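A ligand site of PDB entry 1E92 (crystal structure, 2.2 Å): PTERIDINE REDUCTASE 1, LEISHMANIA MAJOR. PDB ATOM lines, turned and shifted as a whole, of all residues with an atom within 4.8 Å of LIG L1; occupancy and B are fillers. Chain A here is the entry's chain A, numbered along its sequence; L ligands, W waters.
N of Ser 40 lies within hydrogen-bond range of O15 of LIG L1, at 3.0 Å.
OG of Ser 40 lies within hydrogen-bond range of O17 of LIG L1 (2.5 Å).
N of Ser 227 is in hydrogen-bond range of O14 of LIG L1.
A nitrogen (N7) of LIG L1 is in hydrogen-bond range of the backbone carbonyl oxygen (O) of Ser 227, 3.1 Å away.
The side-chain carboxylate (OD1) of Asp 142 is in hydrogen-bond range of a nitrogen (N3) of LIG L1, 2.7 Å away.
N of Arg 39 is in hydrogen-bond range of O16 of LIG L1 (2.7 Å).
The backbone NH (N) of Leu 66 is in hydrogen-bond range of a nitrogen (N4) of LIG L1 (2.8 Å).
An oxygen (O15) of LIG L1 is in hydrogen-bond range of the backbone NH (N) of His 38 (2.8 Å).
The guanidinium group of Arg 17 lies within salt-bridge range of an oxygen (O8) of LIG L1, 2.9 Å away.
NZ of Lys 198 is in hydrogen-bond range of O12 of LIG L1, 2.9 Å away.
The backbone NH (N) of Ser 111 lies within hydrogen-bond range of an oxygen (O4) of LIG L1 (2.9 Å).
OG of Ser 111 is in hydrogen-bond range of O13 of LIG L1, 3.1 Å away.
The backbone carbonyl oxygen of Asn 109 is in hydrogen-bond range of an oxygen (O12) of LIG L1 (2.9 Å).
N of Leu 18 lies within hydrogen-bond range of O9 of LIG L1, at 3.1 Å.
The side-chain carboxylate (OD1) of Asp 65 sits at hydrogen-bond distance from a nitrogen (N3) of LIG L1.
O1 of LG2 L2 is in hydrogen-bond range of NH2 of Arg 17, 3.3 Å away.
N2 of LG2 L2 sits at hydrogen-bond distance from O of Ser 111, 3.0 Å away.
The side-chain hydroxyl (OG) of Ser 111 sits at hydrogen-bond distance from a nitrogen (N2) of LG2 L2.
A nitrogen (N4) of LG2 L2 is in hydrogen-bond range of the side-chain hydroxyl of Tyr 194, 2.7 Å away.
O1 of LIG L1 is in hydrogen-bond range of N3 of LG2 L2, at 2.6 Å.
Water W3 lies within hydrogen-bond range of O16 of LIG L1 (2.7 Å) and ND1 of His 38 (2.9 Å).
Water W8 lies within hydrogen-bond range of the backbone carbonyl oxygen (O) of Gly 13 (2.6 Å), an oxygen (O5) of LIG L1 (2.8 Å) and the backbone NH (N) of Lys 16 (2.9 Å).
Water W7 lies within hydrogen-bond range of N of Ala 15, O15 of LIG L1 and O of His 36.
Water W4 lies within hydrogen-bond range of NZ of Lys 198 (2.9 Å), O12 of LIG L1 (3.0 Å), O of Ala 110 (3.2 Å) and O of Met 179 (3.3 Å).
Water W5 lies within hydrogen-bond range of the side-chain carboxylate of Asp 142 (2.8 Å) and a nitrogen (N2) of LIG L1 (3.2 Å).
Merely in contact with LIG L1: Gly 13 (3.8 Å), Lys 16 (3.9 Å), His 36 (3.7 Å), Tyr 37 (3.5 Å), Ala 64 (3.4 Å), Ser 67 (3.8 Å), Ala 110 (3.3 Å), Ser 112 (3.7 Å), Met 179 (3.5 Å), Val 180 (3.2 Å), Asp 181 (3.6 Å), Tyr 194 (3.7 Å), Pro 224 (3.3 Å), Gly 225 (3.1 Å) and Leu 226 (3.5 Å).
Hydrophobic or aromatic side chains that line LIG L1: Leu 18, His 36, Tyr 37, His 38, Leu 66, Ala 110, Met 179 and Pro 224.
Of the 32 residues printed, 27 come within 4 Å of LIG L1.
The backbone carbonyl oxygen (O) of Asp 142 sits at hydrogen-bond distance from the side-chain hydroxyl (OG) of Ser 146, at 2.9 Å.
The backbone NH of Ser 146 lies within hydrogen-bond range of the backbone carbonyl oxygen of Leu 66.
NZ of Lys 198 sits at hydrogen-bond distance from OD1 of Asn 147, 3.1 Å away.
N of Ala 64 is in hydrogen-bond range of O of Tyr 37 (3.0 Å).
The backbone carbonyl oxygen (O) of Ala 64 sits at hydrogen-bond distance from a ring nitrogen (NE2) of His 36, 2.6 Å away.
OD1 of Asp 65 sits at hydrogen-bond distance from N of Ser 67 (2.9 Å).
The backbone carbonyl oxygen of Ser 112 lies within hydrogen-bond range of the side-chain amide nitrogen of Asn 147 (3.0 Å).
The backbone NH (N) of Gly 13 lies within hydrogen-bond range of a ring nitrogen (ND1) of His 36.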
ATOM      1  N   GLY A  13       8.341  22.636  10.190  1.00  0.00           N
ATOM      2  CA  GLY A  13       8.166  24.079  10.337  1.00  0.00           C
ATOM      3  C   GLY A  13       9.331  24.662  11.129  1.00  0.00           C
ATOM      4  O   GLY A  13       9.147  25.464  12.045  1.00  0.00           O
ATOM      5  N   ALA A  15      11.827  26.715  10.062  1.00  0.00           N
ATOM      6  CA  ALA A  15      12.497  27.941   9.583  1.00  0.00           C
ATOM      7  C   ALA A  15      12.528  29.100  10.543  1.00  0.00           C
ATOM      8  O   ALA A  15      13.455  29.914  10.528  1.00  0.00           O
ATOM      9  CB  ALA A  15      11.892  28.388   8.250  1.00  0.00           C
ATOM     10  N   LYS A  16      11.537  29.190  11.408  1.00  0.00           N
ATOM     11  CA  LYS A  16      11.584  30.291  12.330  1.00  0.00           C
ATOM     12  C   LYS A  16      10.914  30.076  13.638  1.00  0.00           C
ATOM     13  O   LYS A  16      10.528  28.964  13.989  1.00  0.00           O
ATOM     14  CB  LYS A  16      11.002  31.527  11.655  1.00  0.00           C
ATOM     15  CG  LYS A  16       9.876  31.255  10.743  1.00  0.00           C
ATOM     16  CD  LYS A  16       9.628  32.453   9.823  1.00  0.00           C
ATOM     17  CE  LYS A  16       8.268  32.333   9.192  1.00  0.00           C
ATOM     18  NZ  LYS A  16       8.022  33.347   8.132  1.00  0.00           N
ATOM     19  N   ARG A  17      10.843  31.160  14.389  1.00  0.00           N
ATOM     20  CA  ARG A  17      10.152  31.183  15.667  1.00  0.00           C
ATOM     21  C   ARG A  17      10.453  29.960  16.543  1.00  0.00           C
ATOM     22  O   ARG A  17      11.639  29.646  16.739  1.00  0.00           O
ATOM     23  CB  ARG A  17       8.660  31.392  15.369  1.00  0.00           C
ATOM     24  CG  ARG A  17       8.397  32.868  14.838  1.00  0.00           C
ATOM     25  CD  ARG A  17       7.044  33.030  14.161  1.00  0.00           C
ATOM     26  NE  ARG A  17       5.953  32.694  15.087  1.00  0.00           N
ATOM     27  CZ  ARG A  17       5.499  33.516  16.042  1.00  0.00           C
ATOM     28  NH1 ARG A  17       6.034  34.734  16.197  1.00  0.00           N
ATOM     29  NH2 ARG A  17       4.530  33.116  16.852  1.00  0.00           N
ATOM     30  N   LEU A  18       9.434  29.274  17.071  1.00  0.00           N
ATOM     31  CA  LEU A  18       9.704  28.139  17.955  1.00  0.00           C
ATOM     32  C   LEU A  18      10.427  26.962  17.289  1.00  0.00           C
ATOM     33  O   LEU A  18      11.321  26.371  17.894  1.00  0.00           O
ATOM     34  CB  LEU A  18       8.406  27.637  18.634  1.00  0.00           C
ATOM     35  CG  LEU A  18       7.503  28.598  19.466  1.00  0.00           C
ATOM     36  CD1 LEU A  18       6.638  27.819  20.469  1.00  0.00           C
ATOM     37  CD2 LEU A  18       8.317  29.611  20.192  1.00  0.00           C
ATOM     38  N   GLY A  19      10.044  26.619  16.051  1.00  0.00           N
ATOM     39  CA  GLY A  19      10.698  25.515  15.337  1.00  0.00           C
ATOM     40  C   GLY A  19      12.182  25.787  15.147  1.00  0.00           C
ATOM     41  O   GLY A  19      13.018  24.921  15.320  1.00  0.00           O
ATOM     42  N   HIS A  36      12.497  20.977   8.109  1.00  0.00           N
ATOM     43  CA  HIS A  36      11.425  20.965   7.128  1.00  0.00           C
ATOM     44  C   HIS A  36      10.834  22.359   7.049  1.00  0.00           C
ATOM     45  O   HIS A  36      10.838  23.105   8.043  1.00  0.00           O
ATOM     46  CB  HIS A  36      10.312  19.950   7.500  1.00  0.00           C
ATOM     47  CG  HIS A  36       8.974  20.332   6.940  1.00  0.00           C
ATOM     48  ND1 HIS A  36       8.163  21.268   7.545  1.00  0.00           N
ATOM     49  CD2 HIS A  36       8.330  19.931   5.816  1.00  0.00           C
ATOM     50  CE1 HIS A  36       7.062  21.423   6.818  1.00  0.00           C
ATOM     51  NE2 HIS A  36       7.145  20.623   5.760  1.00  0.00           N
ATOM     52  N   TYR A  37      10.356  22.728   5.871  1.00  0.00           N
ATOM     53  CA  TYR A  37       9.728  24.038   5.668  1.00  0.00           C
ATOM     54  C   TYR A  37       8.682  23.899   4.571  1.00  0.00           C
ATOM     55  O   TYR A  37       8.672  22.915   3.811  1.00  0.00           O
ATOM     56  CB  TYR A  37      10.777  25.097   5.279  1.00  0.00           C
ATOM     57  CG  TYR A  37      11.351  24.905   3.879  1.00  0.00           C
ATOM     58  CD1 TYR A  37      10.740  25.491   2.759  1.00  0.00           C
ATOM     59  CD2 TYR A  37      12.478  24.115   3.683  1.00  0.00           C
ATOM     60  CE1 TYR A  37      11.270  25.297   1.483  1.00  0.00           C
ATOM     61  CE2 TYR A  37      13.008  23.912   2.428  1.00  0.00           C
ATOM     62  CZ  TYR A  37      12.396  24.490   1.329  1.00  0.00           C
ATOM     63  OH  TYR A  37      12.923  24.227   0.087  1.00  0.00           O
ATOM     64  N   HIS A  38       7.759  24.853   4.511  1.00  0.00           N
ATOM     65  CA  HIS A  38       6.737  24.806   3.478  1.00  0.00           C
ATOM     66  C   HIS A  38       6.956  26.027   2.561  1.00  0.00           C
ATOM     67  O   HIS A  38       7.337  25.864   1.406  1.00  0.00           O
ATOM     68  CB  HIS A  38       5.340  24.844   4.106  1.00  0.00           C
ATOM     69  CG  HIS A  38       4.211  24.863   3.098  1.00  0.00           C
ATOM     70  ND1 HIS A  38       2.997  25.471   3.350  1.00  0.00           N
ATOM     71  CD2 HIS A  38       4.125  24.332   1.847  1.00  0.00           C
ATOM     72  CE1 HIS A  38       2.217  25.318   2.293  1.00  0.00           C
ATOM     73  NE2 HIS A  38       2.877  24.629   1.375  1.00  0.00           N
ATOM     74  N   ARG A  39       6.756  27.245   3.084  1.00  0.00           N
ATOM     75  CA  ARG A  39       6.940  28.452   2.292  1.00  0.00           C
ATOM     76  C   ARG A  39       8.178  29.266   2.634  1.00  0.00           C
ATOM     77  O   ARG A  39       8.573  30.121   1.875  1.00  0.00           O
ATOM     78  CB  ARG A  39       5.690  29.314   2.402  1.00  0.00           C
ATOM     79  CG  ARG A  39       4.538  28.647   1.633  1.00  0.00           C
ATOM     80  CD  ARG A  39       3.188  29.243   1.887  1.00  0.00           C
ATOM     81  NE  ARG A  39       2.143  28.402   1.300  1.00  0.00           N
ATOM     82  CZ  ARG A  39       0.908  28.341   1.750  1.00  0.00           C
ATOM     83  NH1 ARG A  39       0.544  29.079   2.803  1.00  0.00           N
ATOM     84  NH2 ARG A  39       0.016  27.539   1.169  1.00  0.00           N
ATOM     85  N   SER A  40       8.787  28.990   3.787  1.00  0.00           N
ATOM     86  CA  SER A  40       9.960  29.761   4.207  1.00  0.00           C
ATOM     87  C   SER A  40      11.316  29.201   3.761  1.00  0.00           C
ATOM     88  O   SER A  40      12.224  28.939   4.568  1.00  0.00           O
ATOM     89  CB  SER A  40       9.897  29.912   5.721  1.00  0.00           C
ATOM     90  OG  SER A  40       8.737  30.647   6.052  1.00  0.00           O
ATOM     91  N   ALA A  64       7.846  20.605   2.121  1.00  0.00           N
ATOM     92  CA  ALA A  64       6.622  19.819   2.057  1.00  0.00           C
ATOM     93  C   ALA A  64       5.456  20.551   2.620  1.00  0.00           C
ATOM     94  O   ALA A  64       5.566  21.147   3.705  1.00  0.00           O
ATOM     95  CB  ALA A  64       6.784  18.514   2.808  1.00  0.00           C
ATOM     96  N   ASP A  65       4.354  20.471   1.886  1.00  0.00           N
ATOM     97  CA  ASP A  65       3.080  21.041   2.296  1.00  0.00           C
ATOM     98  C   ASP A  65       2.492  19.894   3.136  1.00  0.00           C
ATOM     99  O   ASP A  65       2.339  18.785   2.645  1.00  0.00           O
ATOM    100  CB  ASP A  65       2.207  21.307   1.074  1.00  0.00           C
ATOM    101  CG  ASP A  65       0.834  21.856   1.452  1.00  0.00           C
ATOM    102  OD1 ASP A  65       0.584  22.036   2.667  1.00  0.00           O
ATOM    103  OD2 ASP A  65       0.009  22.104   0.558  1.00  0.00           O
ATOM    104  N   LEU A  66       2.201  20.149   4.411  1.00  0.00           N
ATOM    105  CA  LEU A  66       1.669  19.105   5.281  1.00  0.00           C
ATOM    106  C   LEU A  66       0.148  19.204   5.384  1.00  0.00           C
ATOM    107  O   LEU A  66      -0.484  18.625   6.288  1.00  0.00           O
ATOM    108  CB  LEU A  66       2.306  19.208   6.663  1.00  0.00           C
ATOM    109  CG  LEU A  66       3.820  19.004   6.657  1.00  0.00           C
ATOM    110  CD1 LEU A  66       4.399  19.113   8.073  1.00  0.00           C
ATOM    111  CD2 LEU A  66       4.152  17.660   6.061  1.00  0.00           C
ATOM    112  N   SER A  67      -0.451  19.967   4.475  1.00  0.00           N
ATOM    113  CA  SER A  67      -1.883  20.089   4.449  1.00  0.00           C
ATOM    114  C   SER A  67      -2.418  18.727   4.001  1.00  0.00           C
ATOM    115  O   SER A  67      -1.719  18.013   3.282  1.00  0.00           O
ATOM    116  CB  SER A  67      -2.310  21.189   3.469  1.00  0.00           C
ATOM    117  OG  SER A  67      -3.695  21.030   3.223  1.00  0.00           O
ATOM    118  N   ASN A 109       6.166  20.292  14.944  1.00  0.00           N
ATOM    119  CA  ASN A 109       5.993  21.687  15.284  1.00  0.00           C
ATOM    120  C   ASN A 109       5.208  22.490  14.237  1.00  0.00           C
ATOM    121  O   ASN A 109       4.507  23.436  14.602  1.00  0.00           O
ATOM    122  CB  ASN A 109       7.371  22.296  15.486  1.00  0.00           C
ATOM    123  CG  ASN A 109       7.352  23.788  15.649  1.00  0.00           C
ATOM    124  OD1 ASN A 109       7.147  24.299  16.752  1.00  0.00           O
ATOM    125  ND2 ASN A 109       7.575  24.523  14.547  1.00  0.00           N
ATOM    126  N   ALA A 110       5.317  22.108  12.943  1.00  0.00           N
ATOM    127  CA  ALA A 110       4.610  22.852  11.873  1.00  0.00           C
ATOM    128  C   ALA A 110       3.132  22.947  12.184  1.00  0.00           C
ATOM    129  O   ALA A 110       2.514  21.963  12.636  1.00  0.00           O
ATOM    130  CB  ALA A 110       4.825  22.186  10.506  1.00  0.00           C
ATOM    131  N   SER A 111       2.535  24.100  11.876  1.00  0.00           N
ATOM    132  CA  SER A 111       1.137  24.304  12.245  1.00  0.00           C
ATOM    133  C   SER A 111       0.502  25.550  11.675  1.00  0.00           C
ATOM    134  O   SER A 111       1.062  26.649  11.823  1.00  0.00           O
ATOM    135  CB  SER A 111       1.050  24.381  13.794  1.00  0.00           C
ATOM    136  OG  SER A 111      -0.068  25.127  14.263  1.00  0.00           O
ATOM    137  N   SER A 112      -0.658  25.407  11.049  1.00  0.00           N
ATOM    138  CA  SER A 112      -1.343  26.595  10.536  1.00  0.00           C
ATOM    139  C   SER A 112      -2.305  27.024  11.632  1.00  0.00           C
ATOM    140  O   SER A 112      -2.806  26.193  12.419  1.00  0.00           O
ATOM    141  CB  SER A 112      -2.072  26.341   9.200  1.00  0.00           C
ATOM    142  OG  SER A 112      -2.920  25.233   9.215  1.00  0.00           O
ATOM    143  N   ASP A 142      -5.922  22.147   5.565  1.00  0.00           N
ATOM    144  CA  ASP A 142      -4.696  22.785   6.008  1.00  0.00           C
ATOM    145  C   ASP A 142      -4.540  22.757   7.545  1.00  0.00           C
ATOM    146  O   ASP A 142      -3.495  22.355   8.088  1.00  0.00           O
ATOM    147  CB  ASP A 142      -4.668  24.229   5.487  1.00  0.00           C
ATOM    148  CG  ASP A 142      -3.399  24.979   5.890  1.00  0.00           C
ATOM    149  OD1 ASP A 142      -2.309  24.443   5.694  1.00  0.00           O
ATOM    150  OD2 ASP A 142      -3.486  26.119   6.378  1.00  0.00           O
ATOM    151  N   SER A 146      -1.740  19.990   9.003  1.00  0.00           N
ATOM    152  CA  SER A 146      -0.518  20.399   9.670  1.00  0.00           C
ATOM    153  C   SER A 146      -0.493  20.068  11.163  1.00  0.00           C
ATOM    154  O   SER A 146       0.506  19.602  11.693  1.00  0.00           O
ATOM    155  CB  SER A 146      -0.290  21.906   9.491  1.00  0.00           C
ATOM    156  OG  SER A 146      -1.341  22.645  10.075  1.00  0.00           O
ATOM    157  N   ASN A 147      -1.614  20.326  11.828  1.00  0.00           N
ATOM    158  CA  ASN A 147      -1.719  20.121  13.263  1.00  0.00           C
ATOM    159  C   ASN A 147      -2.010  18.701  13.754  1.00  0.00           C
ATOM    160  O   ASN A 147      -1.694  18.387  14.922  1.00  0.00           O
ATOM    161  CB  ASN A 147      -2.811  21.044  13.841  1.00  0.00           C
ATOM    162  CG  ASN A 147      -2.416  22.516  13.821  1.00  0.00           C
ATOM    163  OD1 ASN A 147      -1.546  22.935  14.575  1.00  0.00           O
ATOM    164  ND2 ASN A 147      -3.069  23.303  12.956  1.00  0.00           N
ATOM    165  N   MET A 179       3.931  19.497  19.368  1.00  0.00           N
ATOM    166  CA  MET A 179       3.738  20.837  19.904  1.00  0.00           C
ATOM    167  C   MET A 179       2.243  21.063  19.977  1.00  0.00           C
ATOM    168  O   MET A 179       1.569  21.247  18.935  1.00  0.00           O
ATOM    169  CB  MET A 179       4.354  21.902  18.995  1.00  0.00           C
ATOM    170  CG  MET A 179       5.891  21.795  18.842  1.00  0.00           C
ATOM    171  SD  MET A 179       6.760  21.713  20.487  1.00  0.00           S
ATOM    172  CE  MET A 179       6.505  23.400  21.089  1.00  0.00           C
ATOM    173  N   VAL A 180       1.712  21.037  21.195  1.00  0.00           N
ATOM    174  CA  VAL A 180       0.289  21.225  21.395  1.00  0.00           C
ATOM    175  C   VAL A 180      -0.002  22.662  21.833  1.00  0.00           C
ATOM    176  O   VAL A 180       0.715  23.566  21.437  1.00  0.00           O
ATOM    177  CB  VAL A 180      -0.299  20.171  22.382  1.00  0.00           C
ATOM    178  CG1 VAL A 180      -0.292  18.777  21.693  1.00  0.00           C
ATOM    179  CG2 VAL A 180       0.521  20.106  23.688  1.00  0.00           C
ATOM    180  N   ASP A 181      -1.026  22.890  22.653  1.00  0.00           N
ATOM    181  CA  ASP A 181      -1.374  24.273  23.028  1.00  0.00           C
ATOM    182  C   ASP A 181      -1.965  24.295  24.438  1.00  0.00           C
ATOM    183  O   ASP A 181      -3.017  23.729  24.681  1.00  0.00           O
ATOM    184  CB  ASP A 181      -2.398  24.821  22.003  1.00  0.00           C
ATOM    185  CG  ASP A 181      -2.777  26.285  22.255  1.00  0.00           C
ATOM    186  OD1 ASP A 181      -2.567  26.811  23.385  1.00  0.00           O
ATOM    187  OD2 ASP A 181      -3.308  26.907  21.308  1.00  0.00           O
ATOM    188  N   TYR A 194      -8.844  24.760  14.349  1.00  0.00           N
ATOM    189  CA  TYR A 194      -7.520  24.731  14.931  1.00  0.00           C
ATOM    190  C   TYR A 194      -7.579  24.085  16.347  1.00  0.00           C
ATOM    191  O   TYR A 194      -6.735  23.250  16.698  1.00  0.00           O
ATOM    192  CB  TYR A 194      -6.978  26.172  15.063  1.00  0.00           C
ATOM    193  CG  TYR A 194      -5.821  26.238  16.054  1.00  0.00           C
ATOM    194  CD1 TYR A 194      -4.510  25.927  15.658  1.00  0.00           C
ATOM    195  CD2 TYR A 194      -6.056  26.588  17.390  1.00  0.00           C
ATOM    196  CE1 TYR A 194      -3.455  25.970  16.579  1.00  0.00           C
ATOM    197  CE2 TYR A 194      -5.015  26.613  18.322  1.00  0.00           C
ATOM    198  CZ  TYR A 194      -3.734  26.308  17.908  1.00  0.00           C
ATOM    199  OH  TYR A 194      -2.717  26.369  18.830  1.00  0.00           O
ATOM    200  N   LYS A 198      -5.725  20.557  17.518  1.00  0.00           N
ATOM    201  CA  LYS A 198      -4.823  20.402  18.651  1.00  0.00           C
ATOM    202  C   LYS A 198      -5.349  19.311  19.615  1.00  0.00           C
ATOM    203  O   LYS A 198      -4.574  18.585  20.257  1.00  0.00           O
ATOM    204  CB  LYS A 198      -4.623  21.743  19.387  1.00  0.00           C
ATOM    205  CG  LYS A 198      -3.712  22.745  18.640  1.00  0.00           C
ATOM    206  CD  LYS A 198      -2.311  22.140  18.263  1.00  0.00           C
ATOM    207  CE  LYS A 198      -1.350  23.267  17.857  1.00  0.00           C
ATOM    208  NZ  LYS A 198      -0.097  22.750  17.265  1.00  0.00           N
ATOM    209  N   PRO A 224       2.783  25.470  24.510  1.00  0.00           N
ATOM    210  CA  PRO A 224       3.042  26.864  24.867  1.00  0.00           C
ATOM    211  C   PRO A 224       1.706  27.546  25.205  1.00  0.00           C
ATOM    212  O   PRO A 224       0.634  27.032  24.823  1.00  0.00           O
ATOM    213  CB  PRO A 224       3.622  27.458  23.575  1.00  0.00           C
ATOM    214  CG  PRO A 224       4.222  26.253  22.860  1.00  0.00           C
ATOM    215  CD  PRO A 224       3.163  25.187  23.119  1.00  0.00           C
ATOM    216  N   GLY A 225       1.777  28.678  25.922  1.00  0.00           N
ATOM    217  CA  GLY A 225       0.628  29.522  26.227  1.00  0.00           C
ATOM    218  C   GLY A 225       0.708  30.619  25.167  1.00  0.00           C
ATOM    219  O   GLY A 225       0.151  30.509  24.081  1.00  0.00           O
ATOM    220  N   LEU A 226       1.418  31.698  25.476  1.00  0.00           N
ATOM    221  CA  LEU A 226       1.657  32.789  24.525  1.00  0.00           C
ATOM    222  C   LEU A 226       3.177  32.840  24.364  1.00  0.00           C
ATOM    223  O   LEU A 226       3.871  33.038  25.375  1.00  0.00           O
ATOM    224  CB  LEU A 226       1.178  34.122  25.093  1.00  0.00           C
ATOM    225  CG  LEU A 226      -0.304  34.181  25.466  1.00  0.00           C
ATOM    226  CD1 LEU A 226      -0.683  35.612  25.980  1.00  0.00           C
ATOM    227  CD2 LEU A 226      -1.159  33.828  24.245  1.00  0.00           C
ATOM    228  N   SER A 227       3.714  32.659  23.147  1.00  0.00           N
ATOM    229  CA  SER A 227       5.170  32.728  22.910  1.00  0.00           C
ATOM    230  C   SER A 227       5.482  33.570  21.706  1.00  0.00           C
ATOM    231  O   SER A 227       4.823  33.403  20.671  1.00  0.00           O
ATOM    232  CB  SER A 227       5.777  31.360  22.676  1.00  0.00           C
ATOM    233  OG  SER A 227       5.382  30.514  23.726  1.00  0.00           O
ATOM    234  N   VAL A 228       6.491  34.429  21.843  1.00  0.00           N
ATOM    235  CA  VAL A 228       6.881  35.347  20.789  1.00  0.00           C
ATOM    236  C   VAL A 228       5.581  35.804  20.091  1.00  0.00           C
ATOM    237  O   VAL A 228       5.427  35.691  18.894  1.00  0.00           O
ATOM    238  CB  VAL A 228       7.879  34.673  19.814  1.00  0.00           C
ATOM    239  CG1 VAL A 228       9.235  34.412  20.556  1.00  0.00           C
ATOM    240  CG2 VAL A 228       7.331  33.353  19.334  1.00  0.00           C
HETATM  241  P1  LIG L   1       4.107  29.410  13.468  1.00  0.00           P
HETATM  242  O1  LIG L   1       2.707  29.914  13.419  1.00  0.00           O
HETATM  243  O2  LIG L   1       5.166  30.375  13.384  1.00  0.00           O
HETATM  244  O3  LIG L   1       4.256  28.274  12.352  1.00  0.00           O
HETATM  245  C1  LIG L   1       5.248  27.281  12.359  1.00  0.00           C
HETATM  246  C2  LIG L   1       5.514  26.765  10.950  1.00  0.00           C
HETATM  247  O4  LIG L   1       4.486  25.843  10.577  1.00  0.00           O
HETATM  248  C3  LIG L   1       5.446  27.885   9.901  1.00  0.00           C
HETATM  249  O5  LIG L   1       6.743  28.491   9.808  1.00  0.00           O
HETATM  250  C4  LIG L   1       5.103  27.080   8.625  1.00  0.00           C
HETATM  251  O6  LIG L   1       6.283  26.868   7.781  1.00  0.00           O
HETATM  252  C5  LIG L   1       4.529  25.722   9.134  1.00  0.00           C
HETATM  253  N1  LIG L   1       3.287  25.401   8.484  1.00  0.00           N
HETATM  254  C6  LIG L   1       2.050  25.985   8.619  1.00  0.00           C
HETATM  255  N2  LIG L   1       1.160  25.360   7.797  1.00  0.00           N
HETATM  256  C7  LIG L   1       1.857  24.418   7.191  1.00  0.00           C
HETATM  257  C8  LIG L   1       1.418  23.502   6.240  1.00  0.00           C
HETATM  258  N3  LIG L   1       0.146  23.448   5.799  1.00  0.00           N
HETATM  259  N4  LIG L   1       2.326  22.604   5.726  1.00  0.00           N
HETATM  260  C9  LIG L   1       3.618  22.621   6.137  1.00  0.00           C
HETATM  261  N5  LIG L   1       4.046  23.495   7.051  1.00  0.00           N
HETATM  262  C10 LIG L   1       3.167  24.421   7.602  1.00  0.00           C
HETATM  263  O7  LIG L   1       4.317  28.600  14.841  1.00  0.00           O
HETATM  264  P2  LIG L   1       4.938  28.989  16.289  1.00  0.00           P
HETATM  265  O8  LIG L   1       4.298  30.235  16.734  1.00  0.00           O
HETATM  266  O9  LIG L   1       6.433  29.007  16.172  1.00  0.00           O
HETATM  267  O10 LIG L   1       4.492  27.764  17.193  1.00  0.00           O
HETATM  268  C11 LIG L   1       5.158  26.486  17.100  1.00  0.00           C
HETATM  269  C12 LIG L   1       4.214  25.394  17.633  1.00  0.00           C
HETATM  270  O11 LIG L   1       3.782  25.786  18.961  1.00  0.00           O
HETATM  271  C13 LIG L   1       2.941  25.229  16.776  1.00  0.00           C
HETATM  272  O12 LIG L   1       2.525  23.860  16.742  1.00  0.00           O
HETATM  273  C14 LIG L   1       1.896  26.082  17.535  1.00  0.00           C
HETATM  274  O13 LIG L   1       0.530  25.683  17.290  1.00  0.00           O
HETATM  275  C15 LIG L   1       2.319  25.897  18.968  1.00  0.00           C
HETATM  276  N6  LIG L   1       1.856  26.990  19.809  1.00  0.00           N
HETATM  277  C16 LIG L   1       2.454  28.314  19.631  1.00  0.00           C
HETATM  278  C17 LIG L   1       1.998  29.353  20.455  1.00  0.00           C
HETATM  279  C18 LIG L   1       2.557  30.795  20.374  1.00  0.00           C
HETATM  280  O14 LIG L   1       2.234  31.592  21.230  1.00  0.00           O
HETATM  281  N7  LIG L   1       3.380  31.068  19.341  1.00  0.00           N
HETATM  282  C19 LIG L   1       0.986  29.085  21.411  1.00  0.00           C
HETATM  283  C20 LIG L   1       0.394  27.789  21.587  1.00  0.00           C
HETATM  284  C21 LIG L   1       0.839  26.744  20.775  1.00  0.00           C
HETATM  285  P3  LIG L   1       6.760  27.817   6.548  1.00  0.00           P
HETATM  286  O15 LIG L   1       8.041  27.200   6.091  1.00  0.00           O
HETATM  287  O16 LIG L   1       5.686  27.803   5.537  1.00  0.00           O
HETATM  288  O17 LIG L   1       7.030  29.169   7.208  1.00  0.00           O
HETATM  289  N1  LG2 L   2      -0.262  28.348  16.595  1.00  0.00           N
HETATM  290  N2  LG2 L   2       0.815  27.821  14.602  1.00  0.00           N
HETATM  291  C1  LG2 L   2       0.547  28.771  15.616  1.00  0.00           C
HETATM  292  N3  LG2 L   2       1.106  29.987  15.518  1.00  0.00           N
HETATM  293  C2  LG2 L   2       0.855  30.888  16.483  1.00  0.00           C
HETATM  294  O1  LG2 L   2       1.428  32.121  16.382  1.00  0.00           O
HETATM  295  C3  LG2 L   2      -0.013  30.571  17.612  1.00  0.00           C
HETATM  296  C4  LG2 L   2      -0.560  29.211  17.597  1.00  0.00           C
HETATM  297  N4  LG2 L   2      -1.432  28.748  18.683  1.00  0.00           N
HETATM  298  C5  LG2 L   2      -1.904  29.802  19.688  1.00  0.00           C
HETATM  299  C6  LG2 L   2      -1.158  31.188  19.676  1.00  0.00           C
HETATM  300  N5  LG2 L   2      -0.327  31.483  18.682  1.00  0.00           N
HETATM  301  C7  LG2 L   2      -1.416  32.204  20.776  1.00  0.00           C
HETATM  302  O2  LG2 L   2      -0.161  32.927  21.062  1.00  0.00           O
HETATM  303  C8  LG2 L   2      -2.620  33.177  20.426  1.00  0.00           C
HETATM  304  O3  LG2 L   2      -3.297  33.705  21.625  1.00  0.00           O
HETATM  305  C9  LG2 L   2      -2.154  34.397  19.520  1.00  0.00           C
HETATM  306  O   HOH W   1       8.014  27.536  14.552  1.00  0.00           O
HETATM  307  O   HOH W   2       5.559  31.508  10.872  1.00  0.00           O
HETATM  308  O   HOH W   3       3.015  27.416   5.544  1.00  0.00           O
HETATM  309  O   HOH W   4       1.684  21.156  15.666  1.00  0.00           O
HETATM  310  O   HOH W   5      -0.849  26.818   5.745  1.00  0.00           O
HETATM  311  O   HOH W   6       4.824  31.326   7.634  1.00  0.00           O
HETATM  312  O   HOH W   7       9.448  26.214   8.475  1.00  0.00           O
HETATM  313  O   HOH W   8       8.877  27.970  11.559  1.00  0.00           O
